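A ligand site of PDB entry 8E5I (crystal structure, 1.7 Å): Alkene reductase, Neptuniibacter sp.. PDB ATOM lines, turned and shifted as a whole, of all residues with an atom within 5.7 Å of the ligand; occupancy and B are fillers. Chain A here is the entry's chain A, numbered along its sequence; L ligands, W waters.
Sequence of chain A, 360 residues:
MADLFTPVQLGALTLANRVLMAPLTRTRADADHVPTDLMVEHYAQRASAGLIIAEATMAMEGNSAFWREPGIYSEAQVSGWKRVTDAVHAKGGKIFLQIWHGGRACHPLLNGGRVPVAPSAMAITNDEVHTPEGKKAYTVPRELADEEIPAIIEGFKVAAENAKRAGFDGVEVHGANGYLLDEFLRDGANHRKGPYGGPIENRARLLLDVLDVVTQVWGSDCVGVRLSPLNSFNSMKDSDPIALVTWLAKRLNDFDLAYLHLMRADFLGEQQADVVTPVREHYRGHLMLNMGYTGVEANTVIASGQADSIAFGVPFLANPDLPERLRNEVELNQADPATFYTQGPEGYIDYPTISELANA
An oxygen (O9) of the ligand is in hydrogen-bond range of the backbone NH (N) of Gly 313 (2.8 Å).
A nitrogen (N2) of the ligand is in hydrogen-bond range of the side-chain amide oxygen of Gln 98 (2.8 Å).
The backbone NH (N) of Val 314 is in hydrogen-bond range of an oxygen (O7) of the ligand (2.8 Å).
N of Ala 56 sits at hydrogen-bond distance from O2 of the ligand (3.2 Å).
OG1 of Thr 25 sits at hydrogen-bond distance from O2 of the ligand (2.6 Å).
N of Gly 292 sits at hydrogen-bond distance from O8 of the ligand (2.8 Å).
An oxygen (O1) of the ligand lies within hydrogen-bond range of a ring nitrogen (NE2) of His 174.
An oxygen (O3) of the ligand lies within hydrogen-bond range of the backbone carbonyl oxygen (O) of Pro 23 (2.8 Å).
An oxygen (O1) of the ligand sits at hydrogen-bond distance from the side-chain amide nitrogen (ND2) of Asn 177, at 3.4 Å.
A nitrogen (N3) of the ligand lies within hydrogen-bond range of the backbone NH (N) of Thr 25, at 2.7 Å.
NH1 of Arg 226 lies within hydrogen-bond range of O1 of the ligand, 2.7 Å away.
An oxygen (O4) of the ligand lies within hydrogen-bond range of the side-chain amide oxygen of Asn 290.
The side-chain carboxylate of Glu 172 lies within hydrogen-bond range of the side-chain amide nitrogen of Gln 98, at 2.9 Å.
The backbone carbonyl oxygen (O) of Arg 226 lies within hydrogen-bond range of the backbone NH (N) of Ala 176.
The side-chain sulfur of Met 263 lies close to the guanidinium group of Arg 226, at 3.7 Å.
The backbone NH of Ala 176 lies within hydrogen-bond range of a ring nitrogen (ND1) of His 174 (3.2 Å).
O of Ala 311 lies within hydrogen-bond range of ND2 of Asn 290 (3.0 Å).
The backbone carbonyl oxygen (O) of Phe 312 is in hydrogen-bond range of the backbone NH (N) of Ala 22, 2.9 Å away.
The guanidinium group (NH2) of Arg 226 sits at hydrogen-bond distance from the side-chain amide oxygen (OD1) of Asn 290, 3.2 Å away.
The backbone NH of Ala 56 lies within hydrogen-bond range of the side-chain amide oxygen of Gln 98 (3.3 Å).
Ala 22 touches the ligand (CB to O3, 3.4 Å).
CA of Leu 24 touches N3 of the ligand, 3.4 Å away.
Met 263 touches the ligand (CE to O4, 3.8 Å).
CZ of Phe 267 touches C13 of the ligand, 3.7 Å away.
Met 291 touches the ligand (C to O8, 3.7 Å).
Phe 312 touches the ligand (CA to O9, 3.7 Å).
CD of Pro 315 touches O7 of the ligand (3.9 Å).
CD2 of Phe 340 touches C7 of the ligand, at 3.6 Å.
Tyr 341 touches the ligand (OH to C7, 3.3 Å).
Hydrophobic or aromatic side chains within 4 Å of the ligand: Ala 22, Pro 23, Leu 24, Ala 56, His 174, Met 263, Phe 267, Val 314, Pro 315, Phe 340 and Tyr 341.
Within 4 Å of the ligand: Ala 22, Pro 23, Leu 24, Thr 25, Ala 56, Gln 98, His 174, Asn 177, Arg 226, Met 263, Phe 267, Asn 290, Met 291, Gly 292, Phe 312, Gly 313, Val 314, Pro 315, Phe 340 and Tyr 341.
Water W1 bridges O8 of the ligand and N of Gly 292.
Water W3 bridges the backbone carbonyl oxygen of Tyr 293 (2.8 Å) and an oxygen (O9) of the ligand (2.8 Å).
Water W2 lies within hydrogen-bond range of an oxygen (O9) of the ligand, the backbone NH of Met 291, the backbone carbonyl oxygen of Ala 311 and the side-chain amide nitrogen of Asn 290.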
ATOM      1  N   ALA A  22      -3.754  24.103  16.108  1.00  0.00           N
ATOM      2  CA  ALA A  22      -2.510  24.713  16.590  1.00  0.00           C
ATOM      3  C   ALA A  22      -1.473  24.810  15.462  1.00  0.00           C
ATOM      4  O   ALA A  22      -1.529  24.051  14.490  1.00  0.00           O
ATOM      5  CB  ALA A  22      -1.915  23.834  17.699  1.00  0.00           C
ATOM      6  N   PRO A  23      -0.483  25.702  15.602  1.00  0.00           N
ATOM      7  CA  PRO A  23       0.536  25.839  14.530  1.00  0.00           C
ATOM      8  C   PRO A  23       1.429  24.604  14.518  1.00  0.00           C
ATOM      9  O   PRO A  23       1.877  24.162  15.574  1.00  0.00           O
ATOM     10  CB  PRO A  23       1.303  27.102  14.929  1.00  0.00           C
ATOM     11  CG  PRO A  23       1.092  27.192  16.429  1.00  0.00           C
ATOM     12  CD  PRO A  23      -0.321  26.714  16.651  1.00  0.00           C
ATOM     13  N   LEU A  24       1.672  24.046  13.329  1.00  0.00           N
ATOM     14  CA  LEU A  24       2.454  22.806  13.205  1.00  0.00           C
ATOM     15  C   LEU A  24       3.465  22.935  12.072  1.00  0.00           C
ATOM     16  O   LEU A  24       3.071  22.881  10.920  1.00  0.00           O
ATOM     17  CB  LEU A  24       1.544  21.640  12.929  1.00  0.00           C
ATOM     18  CG  LEU A  24       0.546  21.350  14.074  1.00  0.00           C
ATOM     19  CD1 LEU A  24      -0.675  20.585  13.473  1.00  0.00           C
ATOM     20  CD2 LEU A  24       1.299  20.611  15.194  1.00  0.00           C
ATOM     21  N   THR A  25       4.740  23.124  12.427  1.00  0.00           N
ATOM     22  CA  THR A  25       5.854  23.111  11.473  1.00  0.00           C
ATOM     23  C   THR A  25       5.933  21.754  10.771  1.00  0.00           C
ATOM     24  O   THR A  25       6.065  20.747  11.442  1.00  0.00           O
ATOM     25  CB  THR A  25       7.159  23.342  12.254  1.00  0.00           C
ATOM     26  OG1 THR A  25       7.156  24.749  12.652  1.00  0.00           O
ATOM     27  CG2 THR A  25       8.355  23.132  11.404  1.00  0.00           C
ATOM     28  N   ARG A  26       5.839  21.740   9.436  1.00  0.00           N
ATOM     29  CA  ARG A  26       5.883  20.458   8.734  1.00  0.00           C
ATOM     30  C   ARG A  26       6.929  20.466   7.637  1.00  0.00           C
ATOM     31  O   ARG A  26       7.139  19.440   6.978  1.00  0.00           O
ATOM     32  CB  ARG A  26       4.500  20.164   8.105  1.00  0.00           C
ATOM     33  CG  ARG A  26       3.288  20.219   9.102  1.00  0.00           C
ATOM     34  CD  ARG A  26       3.442  19.123  10.166  1.00  0.00           C
ATOM     35  NE  ARG A  26       3.648  17.767   9.674  1.00  0.00           N
ATOM     36  CZ  ARG A  26       2.667  17.008   9.185  1.00  0.00           C
ATOM     37  NH1 ARG A  26       1.410  17.467   9.138  1.00  0.00           N
ATOM     38  NH2 ARG A  26       2.967  15.807   8.682  1.00  0.00           N
ATOM     39  N   GLU A  55       1.628  27.391  10.562  1.00  0.00           N
ATOM     40  CA  GLU A  55       2.895  27.081  11.219  1.00  0.00           C
ATOM     41  C   GLU A  55       3.854  28.281  11.302  1.00  0.00           C
ATOM     42  O   GLU A  55       3.770  29.243  10.521  1.00  0.00           O
ATOM     43  CB  GLU A  55       3.590  25.963  10.429  1.00  0.00           C
ATOM     44  CG  GLU A  55       3.941  26.464   9.018  1.00  0.00           C
ATOM     45  CD  GLU A  55       3.920  25.230   8.034  1.00  0.00           C
ATOM     46  OE1 GLU A  55       2.924  25.078   7.266  1.00  0.00           O
ATOM     47  OE2 GLU A  55       4.882  24.436   8.041  1.00  0.00           O
ATOM     48  N   ALA A  56       4.848  28.150  12.203  1.00  0.00           N
ATOM     49  CA  ALA A  56       5.904  29.135  12.407  1.00  0.00           C
ATOM     50  C   ALA A  56       6.492  29.533  11.046  1.00  0.00           C
ATOM     51  O   ALA A  56       6.930  28.686  10.265  1.00  0.00           O
ATOM     52  CB  ALA A  56       6.998  28.624  13.350  1.00  0.00           C
ATOM     53  N   GLN A  98       1.270  32.345  12.105  1.00  0.00           N
ATOM     54  CA  GLN A  98       2.219  32.524  13.254  1.00  0.00           C
ATOM     55  C   GLN A  98       3.519  33.142  12.743  1.00  0.00           C
ATOM     56  O   GLN A  98       4.205  32.529  11.915  1.00  0.00           O
ATOM     57  CB  GLN A  98       2.515  31.188  13.968  1.00  0.00           C
ATOM     58  CG  GLN A  98       3.328  31.425  15.265  1.00  0.00           C
ATOM     59  CD  GLN A  98       3.676  30.103  15.915  1.00  0.00           C
ATOM     60  OE1 GLN A  98       4.258  29.221  15.260  1.00  0.00           O
ATOM     61  NE2 GLN A  98       3.239  29.915  17.144  1.00  0.00           N
ATOM     62  N   GLU A 172      -0.448  35.547  14.672  1.00  0.00           N
ATOM     63  CA  GLU A 172      -0.107  35.159  16.036  1.00  0.00           C
ATOM     64  C   GLU A 172       1.380  35.434  16.210  1.00  0.00           C
ATOM     65  O   GLU A 172       2.215  34.987  15.416  1.00  0.00           O
ATOM     66  CB  GLU A 172      -0.488  33.704  16.301  1.00  0.00           C
ATOM     67  CG  GLU A 172       0.144  33.163  17.583  1.00  0.00           C
ATOM     68  CD  GLU A 172      -0.285  31.736  17.986  1.00  0.00           C
ATOM     69  OE1 GLU A 172      -1.496  31.406  18.227  1.00  0.00           O
ATOM     70  OE2 GLU A 172       0.611  30.880  17.821  1.00  0.00           O
ATOM     71  N   HIS A 174       4.818  34.696  17.778  1.00  0.00           N
ATOM     72  CA  HIS A 174       5.403  33.494  18.390  1.00  0.00           C
ATOM     73  C   HIS A 174       6.274  33.913  19.580  1.00  0.00           C
ATOM     74  O   HIS A 174       7.469  34.152  19.422  1.00  0.00           O
ATOM     75  CB  HIS A 174       6.232  32.719  17.361  1.00  0.00           C
ATOM     76  CG  HIS A 174       6.505  31.314  17.767  1.00  0.00           C
ATOM     77  ND1 HIS A 174       6.456  30.931  19.084  1.00  0.00           N
ATOM     78  CD2 HIS A 174       6.677  30.191  17.041  1.00  0.00           C
ATOM     79  CE1 HIS A 174       6.643  29.617  19.154  1.00  0.00           C
ATOM     80  NE2 HIS A 174       6.813  29.149  17.930  1.00  0.00           N
ATOM     81  N   ALA A 176       6.930  31.799  22.130  1.00  0.00           N
ATOM     82  CA  ALA A 176       7.011  30.553  22.892  1.00  0.00           C
ATOM     83  C   ALA A 176       8.173  29.686  22.380  1.00  0.00           C
ATOM     84  O   ALA A 176       8.949  30.076  21.497  1.00  0.00           O
ATOM     85  CB  ALA A 176       5.677  29.754  22.792  1.00  0.00           C
ATOM     86  N   ASN A 177       8.348  28.578  23.088  1.00  0.00           N
ATOM     87  CA  ASN A 177       9.167  27.435  22.647  1.00  0.00           C
ATOM     88  C   ASN A 177      10.649  27.763  22.414  1.00  0.00           C
ATOM     89  O   ASN A 177      11.338  27.035  21.664  1.00  0.00           O
ATOM     90  CB  ASN A 177       8.564  26.843  21.376  1.00  0.00           C
ATOM     91  CG  ASN A 177       7.159  26.354  21.627  1.00  0.00           C
ATOM     92  OD1 ASN A 177       6.792  26.079  22.780  1.00  0.00           O
ATOM     93  ND2 ASN A 177       6.344  26.232  20.553  1.00  0.00           N
ATOM     94  N   ARG A 226       1.329  33.692  21.411  1.00  0.00           N
ATOM     95  CA  ARG A 226       1.493  32.375  21.997  1.00  0.00           C
ATOM     96  C   ARG A 226       2.603  32.386  23.064  1.00  0.00           C
ATOM     97  O   ARG A 226       3.700  32.937  22.826  1.00  0.00           O
ATOM     98  CB  ARG A 226       1.811  31.342  20.905  1.00  0.00           C
ATOM     99  CG  ARG A 226       1.623  29.935  21.501  1.00  0.00           C
ATOM    100  CD  ARG A 226       1.685  28.837  20.413  1.00  0.00           C
ATOM    101  NE  ARG A 226       0.813  27.721  20.776  1.00  0.00           N
ATOM    102  CZ  ARG A 226       0.988  26.452  20.387  1.00  0.00           C
ATOM    103  NH1 ARG A 226       2.065  26.103  19.704  1.00  0.00           N
ATOM    104  NH2 ARG A 226       0.012  25.560  20.620  1.00  0.00           N
ATOM    105  N   MET A 263       0.270  27.607  26.188  1.00  0.00           N
ATOM    106  CA  MET A 263       0.604  26.175  26.283  1.00  0.00           C
ATOM    107  C   MET A 263       0.749  25.855  27.761  1.00  0.00           C
ATOM    108  O   MET A 263       1.540  26.516  28.459  1.00  0.00           O
ATOM    109  CB  MET A 263       1.907  25.864  25.535  1.00  0.00           C
ATOM    110  CG  MET A 263       1.818  26.481  24.173  1.00  0.00           C
ATOM    111  SD  MET A 263       3.309  26.399  23.130  1.00  0.00           S
ATOM    112  CE  MET A 263       3.837  24.695  23.302  1.00  0.00           C
ATOM    113  N   PHE A 267       6.729  20.178  27.238  1.00  0.00           N
ATOM    114  CA  PHE A 267       7.040  19.089  26.292  1.00  0.00           C
ATOM    115  C   PHE A 267       7.856  18.000  26.947  1.00  0.00           C
ATOM    116  O   PHE A 267       7.696  16.812  26.625  1.00  0.00           O
ATOM    117  CB  PHE A 267       7.875  19.581  25.091  1.00  0.00           C
ATOM    118  CG  PHE A 267       7.122  20.401  24.029  1.00  0.00           C
ATOM    119  CD1 PHE A 267       5.744  20.581  24.054  1.00  0.00           C
ATOM    120  CD2 PHE A 267       7.851  21.025  22.993  1.00  0.00           C
ATOM    121  CE1 PHE A 267       5.066  21.371  23.064  1.00  0.00           C
ATOM    122  CE2 PHE A 267       7.202  21.811  22.010  1.00  0.00           C
ATOM    123  CZ  PHE A 267       5.805  21.998  22.057  1.00  0.00           C
ATOM    124  N   ASN A 290      -3.755  25.046  25.145  1.00  0.00           N
ATOM    125  CA  ASN A 290      -3.171  23.970  24.348  1.00  0.00           C
ATOM    126  C   ASN A 290      -2.336  23.064  25.233  1.00  0.00           C
ATOM    127  O   ASN A 290      -1.751  23.520  26.229  1.00  0.00           O
ATOM    128  CB  ASN A 290      -2.281  24.553  23.243  1.00  0.00           C
ATOM    129  CG  ASN A 290      -1.437  23.458  22.573  1.00  0.00           C
ATOM    130  OD1 ASN A 290      -0.259  23.304  22.881  1.00  0.00           O
ATOM    131  ND2 ASN A 290      -2.068  22.662  21.677  1.00  0.00           N
ATOM    132  N   MET A 291      -2.278  21.782  24.822  1.00  0.00           N
ATOM    133  CA  MET A 291      -1.362  20.679  25.205  1.00  0.00           C
ATOM    134  C   MET A 291      -2.134  19.534  25.828  1.00  0.00           C
ATOM    135  O   MET A 291      -2.564  19.624  26.974  1.00  0.00           O
ATOM    136  CB  MET A 291      -0.201  21.088  26.157  1.00  0.00           C
ATOM    137  CG  MET A 291       0.731  22.162  25.644  1.00  0.00           C
ATOM    138  SD  MET A 291       2.354  22.286  26.427  1.00  0.00           S
ATOM    139  CE  MET A 291       2.848  20.591  26.613  1.00  0.00           C
ATOM    140  N   GLY A 292      -2.268  18.426  25.089  1.00  0.00           N
ATOM    141  CA  GLY A 292      -2.778  17.212  25.682  1.00  0.00           C
ATOM    142  C   GLY A 292      -4.276  17.157  25.915  1.00  0.00           C
ATOM    143  O   GLY A 292      -4.727  16.253  26.637  1.00  0.00           O
ATOM    144  N   TYR A 293      -5.054  18.057  25.318  1.00  0.00           N
ATOM    145  CA  TYR A 293      -6.507  18.042  25.531  1.00  0.00           C
ATOM    146  C   TYR A 293      -7.149  16.958  24.677  1.00  0.00           C
ATOM    147  O   TYR A 293      -6.873  16.868  23.483  1.00  0.00           O
ATOM    148  CB  TYR A 293      -7.141  19.369  25.168  1.00  0.00           C
ATOM    149  CG  TYR A 293      -6.833  20.406  26.228  1.00  0.00           C
ATOM    150  CD1 TYR A 293      -7.605  20.474  27.411  1.00  0.00           C
ATOM    151  CD2 TYR A 293      -5.792  21.314  26.062  1.00  0.00           C
ATOM    152  CE1 TYR A 293      -7.308  21.397  28.410  1.00  0.00           C
ATOM    153  CE2 TYR A 293      -5.500  22.260  27.053  1.00  0.00           C
ATOM    154  CZ  TYR A 293      -6.257  22.277  28.220  1.00  0.00           C
ATOM    155  OH  TYR A 293      -5.968  23.194  29.218  1.00  0.00           O
ATOM    156  N   ALA A 311      -6.783  24.698  21.271  1.00  0.00           N
ATOM    157  CA  ALA A 311      -6.049  24.439  20.041  1.00  0.00           C
ATOM    158  C   ALA A 311      -5.535  23.023  20.133  1.00  0.00           C
ATOM    159  O   ALA A 311      -5.006  22.623  21.167  1.00  0.00           O
ATOM    160  CB  ALA A 311      -4.883  25.415  19.831  1.00  0.00           C
ATOM    161  N   PHE A 312      -5.765  22.239  19.093  1.00  0.00           N
ATOM    162  CA  PHE A 312      -5.303  20.885  19.034  1.00  0.00           C
ATOM    163  C   PHE A 312      -4.154  20.829  18.043  1.00  0.00           C
ATOM    164  O   PHE A 312      -4.279  21.348  16.927  1.00  0.00           O
ATOM    165  CB  PHE A 312      -6.449  19.948  18.581  1.00  0.00           C
ATOM    166  CG  PHE A 312      -7.635  19.906  19.515  1.00  0.00           C
ATOM    167  CD1 PHE A 312      -8.621  20.906  19.481  1.00  0.00           C
ATOM    168  CD2 PHE A 312      -7.736  18.886  20.447  1.00  0.00           C
ATOM    169  CE1 PHE A 312      -9.708  20.885  20.378  1.00  0.00           C
ATOM    170  CE2 PHE A 312      -8.814  18.808  21.348  1.00  0.00           C
ATOM    171  CZ  PHE A 312      -9.814  19.808  21.315  1.00  0.00           C
ATOM    172  N   GLY A 313      -3.091  20.117  18.423  1.00  0.00           N
ATOM    173  CA  GLY A 313      -1.909  19.957  17.589  1.00  0.00           C
ATOM    174  C   GLY A 313      -1.958  18.614  16.879  1.00  0.00           C
ATOM    175  O   GLY A 313      -2.502  18.522  15.766  1.00  0.00           O
ATOM    176  N   VAL A 314      -1.324  17.559  17.462  1.00  0.00           N
ATOM    177  CA  VAL A 314      -1.222  16.284  16.766  1.00  0.00           C
ATOM    178  C   VAL A 314      -2.577  15.733  16.330  1.00  0.00           C
ATOM    179  O   VAL A 314      -2.662  15.168  15.230  1.00  0.00           O
ATOM    180  CB  VAL A 314      -0.365  15.304  17.591  1.00  0.00           C
ATOM    181  CG1 VAL A 314      -0.278  13.953  16.959  1.00  0.00           C
ATOM    182  CG2 VAL A 314       1.042  15.886  17.713  1.00  0.00           C
ATOM    183  N   PRO A 315      -3.665  15.889  17.105  1.00  0.00           N
ATOM    184  CA  PRO A 315      -4.939  15.317  16.640  1.00  0.00           C
ATOM    185  C   PRO A 315      -5.411  15.964  15.345  1.00  0.00           C
ATOM    186  O   PRO A 315      -6.003  15.263  14.535  1.00  0.00           O
ATOM    187  CB  PRO A 315      -5.890  15.591  17.819  1.00  0.00           C
ATOM    188  CG  PRO A 315      -5.015  15.560  19.012  1.00  0.00           C
ATOM    189  CD  PRO A 315      -3.752  16.286  18.526  1.00  0.00           C
ATOM    190  N   LEU A 317      -3.332  17.459  13.093  1.00  0.00           N
ATOM    191  CA  LEU A 317      -2.380  16.946  12.101  1.00  0.00           C
ATOM    192  C   LEU A 317      -2.917  15.668  11.439  1.00  0.00           C
ATOM    193  O   LEU A 317      -2.833  15.482  10.202  1.00  0.00           O
ATOM    194  CB  LEU A 317      -1.029  16.675  12.775  1.00  0.00           C
ATOM    195  CG  LEU A 317       0.159  16.189  11.977  1.00  0.00           C
ATOM    196  CD1 LEU A 317       1.534  16.698  12.599  1.00  0.00           C
ATOM    197  CD2 LEU A 317       0.149  14.671  11.791  1.00  0.00           C
ATOM    198  N   PHE A 340       6.324  13.688  10.365  1.00  0.00           N
ATOM    199  CA  PHE A 340       6.063  15.079  10.774  1.00  0.00           C
ATOM    200  C   PHE A 340       6.893  16.039   9.915  1.00  0.00           C
ATOM    201  O   PHE A 340       6.380  17.056   9.438  1.00  0.00           O
ATOM    202  CB  PHE A 340       6.425  15.287  12.238  1.00  0.00           C
ATOM    203  CG  PHE A 340       5.394  14.751  13.229  1.00  0.00           C
ATOM    204  CD1 PHE A 340       4.235  14.164  12.792  1.00  0.00           C
ATOM    205  CD2 PHE A 340       5.649  14.756  14.620  1.00  0.00           C
ATOM    206  CE1 PHE A 340       3.302  13.617  13.703  1.00  0.00           C
ATOM    207  CE2 PHE A 340       4.711  14.247  15.515  1.00  0.00           C
ATOM    208  CZ  PHE A 340       3.541  13.706  15.054  1.00  0.00           C
ATOM    209  N   TYR A 341       8.189  15.723   9.691  1.00  0.00           N
ATOM    210  CA  TYR A 341       9.088  16.694   9.089  1.00  0.00           C
ATOM    211  C   TYR A 341       9.719  16.195   7.793  1.00  0.00           C
ATOM    212  O   TYR A 341      10.761  16.703   7.394  1.00  0.00           O
ATOM    213  CB  TYR A 341      10.199  17.086  10.065  1.00  0.00           C
ATOM    214  CG  TYR A 341       9.714  17.483  11.428  1.00  0.00           C
ATOM    215  CD1 TYR A 341       8.992  18.680  11.634  1.00  0.00           C
ATOM    216  CD2 TYR A 341       9.971  16.657  12.532  1.00  0.00           C
ATOM    217  CE1 TYR A 341       8.561  19.026  12.877  1.00  0.00           C
ATOM    218  CE2 TYR A 341       9.503  17.000  13.767  1.00  0.00           C
ATOM    219  CZ  TYR A 341       8.806  18.199  13.931  1.00  0.00           C
ATOM    220  OH  TYR A 341       8.350  18.591  15.161  1.00  0.00           O
HETATM  221  N1  LIG L   1       4.196  25.147  18.071  1.00  0.00           N
HETATM  222  C1  LIG L   1       4.353  26.385  17.571  1.00  0.00           C
HETATM  223  O1  LIG L   1       4.099  27.322  18.315  1.00  0.00           O
HETATM  224  N2  LIG L   1       4.717  26.615  16.282  1.00  0.00           N
HETATM  225  C2  LIG L   1       5.014  25.546  15.450  1.00  0.00           C
HETATM  226  O2  LIG L   1       5.339  25.761  14.294  1.00  0.00           O
HETATM  227  C3  LIG L   1       4.901  24.254  15.951  1.00  0.00           C
HETATM  228  N3  LIG L   1       5.227  23.210  15.109  1.00  0.00           N
HETATM  229  C4  LIG L   1       5.010  21.903  15.587  1.00  0.00           C
HETATM  230  C5  LIG L   1       5.220  20.829  14.681  1.00  0.00           C
HETATM  231  C6  LIG L   1       4.975  19.526  15.152  1.00  0.00           C
HETATM  232  C7  LIG L   1       5.221  18.343  14.211  1.00  0.00           C
HETATM  233  C8  LIG L   1       4.533  19.343  16.472  1.00  0.00           C
HETATM  234  C9  LIG L   1       4.270  17.982  17.050  1.00  0.00           C
HETATM  235  C10 LIG L   1       4.246  20.402  17.333  1.00  0.00           C
HETATM  236  C11 LIG L   1       4.514  21.709  16.870  1.00  0.00           C
HETATM  237  N4  LIG L   1       4.271  22.791  17.730  1.00  0.00           N
HETATM  238  C12 LIG L   1       4.467  24.045  17.238  1.00  0.00           C
HETATM  239  C13 LIG L   1       3.654  22.555  19.070  1.00  0.00           C
HETATM  240  C14 LIG L   1       2.107  22.450  18.686  1.00  0.00           C
HETATM  241  O3  LIG L   1       1.443  23.670  18.274  1.00  0.00           O
HETATM  242  C15 LIG L   1       1.308  21.930  19.911  1.00  0.00           C
HETATM  243  O4  LIG L   1       1.496  22.846  20.969  1.00  0.00           O
HETATM  244  C16 LIG L   1       1.766  20.567  20.417  1.00  0.00           C
HETATM  245  O5  LIG L   1       1.617  19.603  19.371  1.00  0.00           O
HETATM  246  C17 LIG L   1       0.963  20.068  21.654  1.00  0.00           C
HETATM  247  O6  LIG L   1      -0.448  20.095  21.364  1.00  0.00           O
HETATM  248  P1  LIG L   1      -1.319  18.770  21.290  1.00  0.00           P
HETATM  249  O7  LIG L   1      -0.659  17.935  20.199  1.00  0.00           O
HETATM  250  O8  LIG L   1      -1.123  18.021  22.568  1.00  0.00           O
HETATM  251  O9  LIG L   1      -2.754  19.115  20.994  1.00  0.00           O
HETATM  252  O   HOH W   1       0.882  17.593  24.129  1.00  0.00           O
HETATM  253  O   HOH W   2      -4.148  20.544  23.027  1.00  0.00           O
HETATM  254  O   HOH W   3      -4.506  17.227  22.098  1.00  0.00           O
HETATM  255  O   HOH W   4       0.605  15.717  21.012  1.00  0.00           O
